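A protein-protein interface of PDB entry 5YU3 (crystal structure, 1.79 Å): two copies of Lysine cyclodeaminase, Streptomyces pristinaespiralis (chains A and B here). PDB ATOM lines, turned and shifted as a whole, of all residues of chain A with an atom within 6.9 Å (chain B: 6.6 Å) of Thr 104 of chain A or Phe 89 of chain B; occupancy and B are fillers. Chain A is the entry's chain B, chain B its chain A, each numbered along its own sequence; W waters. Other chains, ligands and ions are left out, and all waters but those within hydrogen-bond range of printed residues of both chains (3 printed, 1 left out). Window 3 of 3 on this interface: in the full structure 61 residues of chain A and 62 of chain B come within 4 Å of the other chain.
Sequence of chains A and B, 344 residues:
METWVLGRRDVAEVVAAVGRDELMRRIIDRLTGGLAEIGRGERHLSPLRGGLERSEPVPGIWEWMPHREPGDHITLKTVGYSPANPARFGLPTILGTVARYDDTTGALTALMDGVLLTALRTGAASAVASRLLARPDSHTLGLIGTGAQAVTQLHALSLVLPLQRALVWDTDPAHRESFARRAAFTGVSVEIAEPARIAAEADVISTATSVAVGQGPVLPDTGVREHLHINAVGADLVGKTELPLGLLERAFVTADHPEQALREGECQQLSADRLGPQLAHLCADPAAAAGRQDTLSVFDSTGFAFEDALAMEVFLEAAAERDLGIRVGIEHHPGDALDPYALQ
The backbone carbonyl oxygen of Thr 104 of chain A is in hydrogen-bond range of the guanidinium group of Arg 54 of chain B (3.3 Å).
O of Thr 105 of chain A is in hydrogen-bond range of ND2 of Asn 85 of chain B, 3.0 Å away.
The side-chain hydroxyl of Ser 82 of chain B lies within hydrogen-bond range of the backbone carbonyl oxygen of Thr 105 of chain A.
The guanidinium group of Arg 54 of chain B lies within hydrogen-bond range of the backbone carbonyl oxygen of Asp 103 of chain A (2.7 Å).
N of Thr 104 of chain A sits at hydrogen-bond distance from OD2 of Asp 102 of chain A (3.1 Å).
The side-chain carboxylate (OD2) of Asp 102 of chain A is in hydrogen-bond range of the backbone NH (N) of Thr 105 of chain A.
The backbone NH (N) of Leu 91 of chain B sits at hydrogen-bond distance from the backbone carbonyl oxygen (O) of Asn 85 of chain B, at 3.2 Å.
N of Asp 103 of chain A is in hydrogen-bond range of O of Asp 72 of chain A (3.0 Å).
The side-chain hydroxyl (OG) of Ser 82 of chain B sits at hydrogen-bond distance from the guanidinium group (NH2) of Arg 54 of chain B (2.7 Å).
The backbone NH of Gly 71 of chain A lies within hydrogen-bond range of the side-chain carboxylate of Asp 103 of chain A, at 2.7 Å.
OG of Ser 82 of chain B touches O of Thr 104 of chain A (3.9 Å).
CG2 of Thr 104 of chain A touches CZ of Phe 89 of chain B (3.6 Å).
Thr 105 of chain A touches Phe 89 of chain B (CG2 to CD2, 3.7 Å).
Leu 91 of chain B touches Thr 105 of chain A.
Arg 54 of chain B touches Gly 106 of chain A.
Pro 86 of chain B touches Ala 337 of chain A (CB to CB, 3.997 Å).
O of Gly 90 of chain B touches CB of Ala 337 of chain A, 3.9 Å away.
O of Leu 91 of chain B touches CB of Ala 337 of chain A, at 3.4 Å.
Of chain B, only Arg 54 (3.3 Å), Ser 82 (3.9 Å) and Phe 89 (3.6 Å) come within 4 Å of Thr 104 of chain A.
Printed residues of chain B within 4 Å of Gly 106 of chain A: Arg 54 (3.9 Å).
Ala 107 of chain A touches none of the printed residues of chain B.
Of chain A, only Thr 104 and Thr 105 come within 4 Å of Phe 89 of chain B.
Printed residues of chain A within 4 Å of Gly 90 of chain B: Ala 337 (3.9 Å).
The nearest printed residue of chain B that does not touch Asp 103 of chain A is Glu 56 of chain B (5.1 Å).
Of the 12 printed residues of chain B, 7 touch a printed residue of chain A.
Hydrophobic or aromatic side chains of chain B that line the printed part of chain A: Pro 86, Phe 89 and Leu 91.
Of the 12 printed residues of chain A, 5 touch a printed residue of chain B.
Printed residues of chain A that touch a printed residue of chain B: Asp 103, Thr 104, Thr 105, Gly 106 and Ala 337.
Hydrophobic or aromatic side chains of chain A that line the printed part of chain B: Ala 337.
Among the printed residues, 12 pairs touch across the chains.
Among the printed residues, no Asp or Glu carboxylate lies within 4 Å of a Lys or Arg side-chain nitrogen of the other chain.
No position is printed for both chains.
Of the 12 pairs that touch across the chains among the printed residues, none has its exchanged pair printed and touching as well.
Water W3 lies within hydrogen-bond range of the side-chain carboxylate of Asp 103 of chain A and the backbone carbonyl oxygen of Glu 56 of chain B.
Water W2 bridges the side-chain hydroxyl (OG) of Ser 82 of chain B (2.8 Å) and the backbone carbonyl oxygen (O) of Thr 105 of chain A (2.9 Å).
Water W1 bridges the side-chain amide oxygen of Asn 85 of chain B (2.9 Å) and the backbone carbonyl oxygen of Thr 104 of chain A (2.9 Å).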
ATOM      1  N   GLY A  71     -16.578  -0.817  31.652  1.00  0.00           N
ATOM      2  CA  GLY A  71     -15.925  -1.516  32.737  1.00  0.00           C
ATOM      3  C   GLY A  71     -16.622  -2.772  33.206  1.00  0.00           C
ATOM      4  O   GLY A  71     -16.050  -3.514  34.018  1.00  0.00           O
ATOM      5  N   ASP A  72     -17.842  -3.032  32.736  1.00  0.00           N
ATOM      6  CA  ASP A  72     -18.603  -4.195  33.160  1.00  0.00           C
ATOM      7  C   ASP A  72     -18.755  -5.149  31.987  1.00  0.00           C
ATOM      8  O   ASP A  72     -17.969  -6.093  31.841  1.00  0.00           O
ATOM      9  CB  ASP A  72     -19.975  -3.785  33.712  1.00  0.00           C
ATOM     10  CG  ASP A  72     -19.872  -2.950  34.979  1.00  0.00           C
ATOM     11  OD1 ASP A  72     -18.846  -3.053  35.689  1.00  0.00           O
ATOM     12  OD2 ASP A  72     -20.819  -2.183  35.265  1.00  0.00           O
ATOM     13  N   HIS A  73     -19.738  -4.898  31.127  1.00  0.00           N
ATOM     14  CA  HIS A  73     -19.987  -5.822  30.039  1.00  0.00           C
ATOM     15  C   HIS A  73     -20.602  -5.104  28.852  1.00  0.00           C
ATOM     16  O   HIS A  73     -21.106  -3.981  28.955  1.00  0.00           O
ATOM     17  CB  HIS A  73     -20.901  -6.965  30.475  1.00  0.00           C
ATOM     18  CG  HIS A  73     -22.054  -6.517  31.311  1.00  0.00           C
ATOM     19  ND1 HIS A  73     -23.192  -5.959  30.770  1.00  0.00           N
ATOM     20  CD2 HIS A  73     -22.236  -6.523  32.654  1.00  0.00           C
ATOM     21  CE1 HIS A  73     -24.035  -5.657  31.742  1.00  0.00           C
ATOM     22  NE2 HIS A  73     -23.474  -5.978  32.895  1.00  0.00           N
ATOM     23  N   ILE A  74     -20.548  -5.790  27.718  1.00  0.00           N
ATOM     24  CA  ILE A  74     -21.185  -5.367  26.480  1.00  0.00           C
ATOM     25  C   ILE A  74     -22.289  -6.365  26.185  1.00  0.00           C
ATOM     26  O   ILE A  74     -22.083  -7.577  26.309  1.00  0.00           O
ATOM     27  CB  ILE A  74     -20.180  -5.304  25.318  1.00  0.00           C
ATOM     28  CG1 ILE A  74     -19.136  -4.222  25.575  1.00  0.00           C
ATOM     29  CG2 ILE A  74     -20.902  -5.050  23.992  1.00  0.00           C
ATOM     30  CD1 ILE A  74     -17.952  -4.309  24.649  1.00  0.00           C
ATOM     31  N   TYR A 101     -20.647  -9.915  26.806  1.00  0.00           N
ATOM     32  CA  TYR A 101     -19.199  -9.966  26.654  1.00  0.00           C
ATOM     33  C   TYR A 101     -18.562  -9.152  27.771  1.00  0.00           C
ATOM     34  O   TYR A 101     -19.046  -8.073  28.117  1.00  0.00           O
ATOM     35  CB  TYR A 101     -18.743  -9.414  25.281  1.00  0.00           C
ATOM     36  CG  TYR A 101     -19.421 -10.067  24.098  1.00  0.00           C
ATOM     37  CD1 TYR A 101     -20.708  -9.693  23.720  1.00  0.00           C
ATOM     38  CD2 TYR A 101     -18.785 -11.067  23.368  1.00  0.00           C
ATOM     39  CE1 TYR A 101     -21.346 -10.297  22.655  1.00  0.00           C
ATOM     40  CE2 TYR A 101     -19.418 -11.680  22.291  1.00  0.00           C
ATOM     41  CZ  TYR A 101     -20.701 -11.284  21.938  1.00  0.00           C
ATOM     42  OH  TYR A 101     -21.358 -11.875  20.873  1.00  0.00           O
ATOM     43  N   ASP A 102     -17.471  -9.662  28.330  1.00  0.00           N
ATOM     44  CA  ASP A 102     -16.757  -8.903  29.346  1.00  0.00           C
ATOM     45  C   ASP A 102     -16.148  -7.653  28.720  1.00  0.00           C
ATOM     46  O   ASP A 102     -15.437  -7.736  27.718  1.00  0.00           O
ATOM     47  CB  ASP A 102     -15.670  -9.766  29.993  1.00  0.00           C
ATOM     48  CG  ASP A 102     -14.918  -9.018  31.072  1.00  0.00           C
ATOM     49  OD1 ASP A 102     -15.467  -8.884  32.181  1.00  0.00           O
ATOM     50  OD2 ASP A 102     -13.794  -8.536  30.810  1.00  0.00           O
ATOM     51  N   ASP A 103     -16.435  -6.486  29.300  1.00  0.00           N
ATOM     52  CA  ASP A 103     -15.970  -5.248  28.678  1.00  0.00           C
ATOM     53  C   ASP A 103     -14.452  -5.111  28.733  1.00  0.00           C
ATOM     54  O   ASP A 103     -13.853  -4.515  27.831  1.00  0.00           O
ATOM     55  CB  ASP A 103     -16.625  -4.039  29.341  1.00  0.00           C
ATOM     56  CG  ASP A 103     -16.294  -2.753  28.629  1.00  0.00           C
ATOM     57  OD1 ASP A 103     -16.582  -2.672  27.416  1.00  0.00           O
ATOM     58  OD2 ASP A 103     -15.733  -1.834  29.274  1.00  0.00           O
ATOM     59  N   THR A 104     -13.817  -5.652  29.774  1.00  0.00           N
ATOM     60  CA  THR A 104     -12.377  -5.478  29.934  1.00  0.00           C
ATOM     61  C   THR A 104     -11.602  -6.303  28.909  1.00  0.00           C
ATOM     62  O   THR A 104     -10.683  -5.794  28.255  1.00  0.00           O
ATOM     63  CB  THR A 104     -11.966  -5.852  31.360  1.00  0.00           C
ATOM     64  OG1 THR A 104     -12.674  -5.019  32.290  1.00  0.00           O
ATOM     65  CG2 THR A 104     -10.455  -5.655  31.563  1.00  0.00           C
ATOM     66  N   THR A 105     -11.973  -7.578  28.746  1.00  0.00           N
ATOM     67  CA  THR A 105     -11.219  -8.512  27.921  1.00  0.00           C
ATOM     68  C   THR A 105     -11.862  -8.825  26.579  1.00  0.00           C
ATOM     69  O   THR A 105     -11.171  -9.341  25.689  1.00  0.00           O
ATOM     70  CB  THR A 105     -11.019  -9.841  28.670  1.00  0.00           C
ATOM     71  OG1 THR A 105     -12.290 -10.476  28.869  1.00  0.00           O
ATOM     72  CG2 THR A 105     -10.368  -9.593  30.013  1.00  0.00           C
ATOM     73  N   GLY A 106     -13.161  -8.566  26.421  1.00  0.00           N
ATOM     74  CA  GLY A 106     -13.890  -9.008  25.250  1.00  0.00           C
ATOM     75  C   GLY A 106     -14.483 -10.401  25.329  1.00  0.00           C
ATOM     76  O   GLY A 106     -15.195 -10.800  24.400  1.00  0.00           O
ATOM     77  N   ALA A 107     -14.225 -11.155  26.397  1.00  0.00           N
ATOM     78  CA  ALA A 107     -14.612 -12.564  26.428  1.00  0.00           C
ATOM     79  C   ALA A 107     -16.130 -12.738  26.453  1.00  0.00           C
ATOM     80  O   ALA A 107     -16.842 -12.031  27.168  1.00  0.00           O
ATOM     81  CB  ALA A 107     -13.997 -13.253  27.644  1.00  0.00           C
ATOM     82  N   ALA A 337      -0.807 -16.819  24.940  1.00  0.00           N
ATOM     83  CA  ALA A 337      -1.691 -15.808  24.364  1.00  0.00           C
ATOM     84  C   ALA A 337      -1.184 -15.270  23.029  1.00  0.00           C
ATOM     85  O   ALA A 337      -1.975 -14.702  22.265  1.00  0.00           O
ATOM     86  CB  ALA A 337      -1.881 -14.657  25.349  1.00  0.00           C
ATOM     87  N   ARG B  54     -13.111   1.308  23.784  1.00  0.00           N
ATOM     88  CA  ARG B  54     -12.938   1.063  25.212  1.00  0.00           C
ATOM     89  C   ARG B  54     -11.577   1.609  25.620  1.00  0.00           C
ATOM     90  O   ARG B  54     -10.568   1.304  24.979  1.00  0.00           O
ATOM     91  CB  ARG B  54     -13.039  -0.445  25.548  1.00  0.00           C
ATOM     92  CG  ARG B  54     -14.401  -1.103  25.247  1.00  0.00           C
ATOM     93  CD  ARG B  54     -14.315  -2.642  25.335  1.00  0.00           C
ATOM     94  NE  ARG B  54     -13.391  -3.097  24.333  1.00  0.00           N
ATOM     95  CZ  ARG B  54     -12.499  -4.074  24.465  1.00  0.00           C
ATOM     96  NH1 ARG B  54     -12.383  -4.800  25.576  1.00  0.00           N
ATOM     97  NH2 ARG B  54     -11.703  -4.313  23.445  1.00  0.00           N
ATOM     98  N   GLU B  56     -10.065   1.534  28.916  1.00  0.00           N
ATOM     99  CA  GLU B  56      -9.395   0.820  29.996  1.00  0.00           C
ATOM    100  C   GLU B  56      -9.249  -0.658  29.662  1.00  0.00           C
ATOM    101  O   GLU B  56     -10.163  -1.248  29.079  1.00  0.00           O
ATOM    102  CB  GLU B  56     -10.169   0.946  31.314  1.00  0.00           C
ATOM    103  CG  GLU B  56     -10.487   2.363  31.702  1.00  0.00           C
ATOM    104  CD  GLU B  56      -9.241   3.209  31.764  1.00  0.00           C
ATOM    105  OE1 GLU B  56      -8.224   2.719  32.306  1.00  0.00           O
ATOM    106  OE2 GLU B  56      -9.271   4.352  31.256  1.00  0.00           O
ATOM    107  N   PRO B  57      -8.141  -1.300  30.072  1.00  0.00           N
ATOM    108  CA  PRO B  57      -6.924  -0.693  30.859  1.00  0.00           C
ATOM    109  C   PRO B  57      -6.029   0.101  29.849  1.00  0.00           C
ATOM    110  O   PRO B  57      -5.235   0.980  30.266  1.00  0.00           O
ATOM    111  CB  PRO B  57      -6.333  -1.706  31.369  1.00  0.00           C
ATOM    112  CG  PRO B  57      -6.709  -2.982  30.459  1.00  0.00           C
ATOM    113  CD  PRO B  57      -7.927  -2.791  30.041  1.00  0.00           C
ATOM    114  N   SER B  82      -8.069  -5.957  22.444  1.00  0.00           N
ATOM    115  CA  SER B  82      -7.793  -5.560  23.827  1.00  0.00           C
ATOM    116  C   SER B  82      -6.318  -5.815  24.079  1.00  0.00           C
ATOM    117  O   SER B  82      -5.928  -6.868  24.603  1.00  0.00           O
ATOM    118  CB  SER B  82      -8.677  -6.329  24.816  1.00  0.00           C
ATOM    119  OG  SER B  82     -10.050  -6.279  24.419  1.00  0.00           O
ATOM    120  N   ALA B  84      -3.965  -5.114  26.067  1.00  0.00           N
ATOM    121  CA  ALA B  84      -3.406  -5.496  27.354  1.00  0.00           C
ATOM    122  C   ALA B  84      -3.760  -6.923  27.749  1.00  0.00           C
ATOM    123  O   ALA B  84      -3.285  -7.389  28.786  1.00  0.00           O
ATOM    124  CB  ALA B  84      -3.869  -4.537  28.457  1.00  0.00           C
ATOM    125  N   ASN B  85      -4.575  -7.625  26.953  1.00  0.00           N
ATOM    126  CA  ASN B  85      -4.981  -8.981  27.321  1.00  0.00           C
ATOM    127  C   ASN B  85      -3.801  -9.910  27.581  1.00  0.00           C
ATOM    128  O   ASN B  85      -3.809 -10.599  28.614  1.00  0.00           O
ATOM    129  CB  ASN B  85      -5.900  -9.564  26.237  1.00  0.00           C
ATOM    130  CG  ASN B  85      -7.373  -9.345  26.540  1.00  0.00           C
ATOM    131  OD1 ASN B  85      -7.720  -8.648  27.490  1.00  0.00           O
ATOM    132  ND2 ASN B  85      -8.245  -9.940  25.725  1.00  0.00           N
ATOM    133  N   PRO B  86      -2.783  -9.998  26.712  1.00  0.00           N
ATOM    134  CA  PRO B  86      -1.711 -10.983  26.962  1.00  0.00           C
ATOM    135  C   PRO B  86      -0.980 -10.755  28.272  1.00  0.00           C
ATOM    136  O   PRO B  86      -0.864 -11.682  29.089  1.00  0.00           O
ATOM    137  CB  PRO B  86      -0.807 -10.826  25.733  1.00  0.00           C
ATOM    138  CG  PRO B  86      -1.846 -10.267  24.635  1.00  0.00           C
ATOM    139  CD  PRO B  86      -2.616  -9.448  25.307  1.00  0.00           C
ATOM    140  N   ALA B  87      -0.517  -9.526  28.511  1.00  0.00           N
ATOM    141  CA  ALA B  87       0.286  -9.233  29.696  1.00  0.00           C
ATOM    142  C   ALA B  87      -0.548  -9.271  30.970  1.00  0.00           C
ATOM    143  O   ALA B  87      -0.083  -9.767  32.003  1.00  0.00           O
ATOM    144  CB  ALA B  87       0.960  -7.865  29.545  1.00  0.00           C
ATOM    145  N   ARG B  88      -1.773  -8.744  30.928  1.00  0.00           N
ATOM    146  CA  ARG B  88      -2.568  -8.601  32.146  1.00  0.00           C
ATOM    147  C   ARG B  88      -3.370  -9.846  32.507  1.00  0.00           C
ATOM    148  O   ARG B  88      -3.520 -10.152  33.695  1.00  0.00           O
ATOM    149  CB  ARG B  88      -3.528  -7.420  32.014  1.00  0.00           C
ATOM    150  CG  ARG B  88      -2.861  -6.077  32.093  1.00  0.00           C
ATOM    151  CD  ARG B  88      -3.780  -5.112  32.788  1.00  0.00           C
ATOM    152  NE  ARG B  88      -3.199  -3.781  32.881  1.00  0.00           N
ATOM    153  CZ  ARG B  88      -3.679  -2.826  33.665  1.00  0.00           C
ATOM    154  NH1 ARG B  88      -4.744  -3.071  34.419  1.00  0.00           N
ATOM    155  NH2 ARG B  88      -3.095  -1.633  33.697  1.00  0.00           N
ATOM    156  N   PHE B  89      -3.912 -10.564  31.519  1.00  0.00           N
ATOM    157  CA  PHE B  89      -4.847 -11.649  31.785  1.00  0.00           C
ATOM    158  C   PHE B  89      -4.452 -12.980  31.160  1.00  0.00           C
ATOM    159  O   PHE B  89      -5.170 -13.965  31.351  1.00  0.00           O
ATOM    160  CB  PHE B  89      -6.255 -11.267  31.298  1.00  0.00           C
ATOM    161  CG  PHE B  89      -6.765  -9.976  31.875  1.00  0.00           C
ATOM    162  CD1 PHE B  89      -7.128  -9.897  33.214  1.00  0.00           C
ATOM    163  CD2 PHE B  89      -6.880  -8.843  31.090  1.00  0.00           C
ATOM    164  CE1 PHE B  89      -7.595  -8.707  33.752  1.00  0.00           C
ATOM    165  CE2 PHE B  89      -7.342  -7.652  31.622  1.00  0.00           C
ATOM    166  CZ  PHE B  89      -7.701  -7.585  32.956  1.00  0.00           C
ATOM    167  N   GLY B  90      -3.354 -13.041  30.414  1.00  0.00           N
ATOM    168  CA  GLY B  90      -3.025 -14.271  29.720  1.00  0.00           C
ATOM    169  C   GLY B  90      -4.002 -14.640  28.633  1.00  0.00           C
ATOM    170  O   GLY B  90      -4.113 -15.818  28.273  1.00  0.00           O
ATOM    171  N   LEU B  91      -4.728 -13.665  28.109  1.00  0.00           N
ATOM    172  CA  LEU B  91      -5.692 -13.861  27.044  1.00  0.00           C
ATOM    173  C   LEU B  91      -5.170 -13.247  25.758  1.00  0.00           C
ATOM    174  O   LEU B  91      -4.333 -12.339  25.785  1.00  0.00           O
ATOM    175  CB  LEU B  91      -7.041 -13.221  27.410  1.00  0.00           C
ATOM    176  CG  LEU B  91      -7.907 -13.952  28.447  1.00  0.00           C
ATOM    177  CD1 LEU B  91      -9.048 -13.068  28.919  1.00  0.00           C
ATOM    178  CD2 LEU B  91      -8.443 -15.261  27.868  1.00  0.00           C
HETATM  179  O   HOH W   1      -7.755  -5.921  28.465  1.00  0.00           O
HETATM  180  O   HOH W   2     -10.404  -8.632  23.025  1.00  0.00           O
HETATM  181  O   HOH W   3     -13.002  -1.676  29.468  1.00  0.00           O
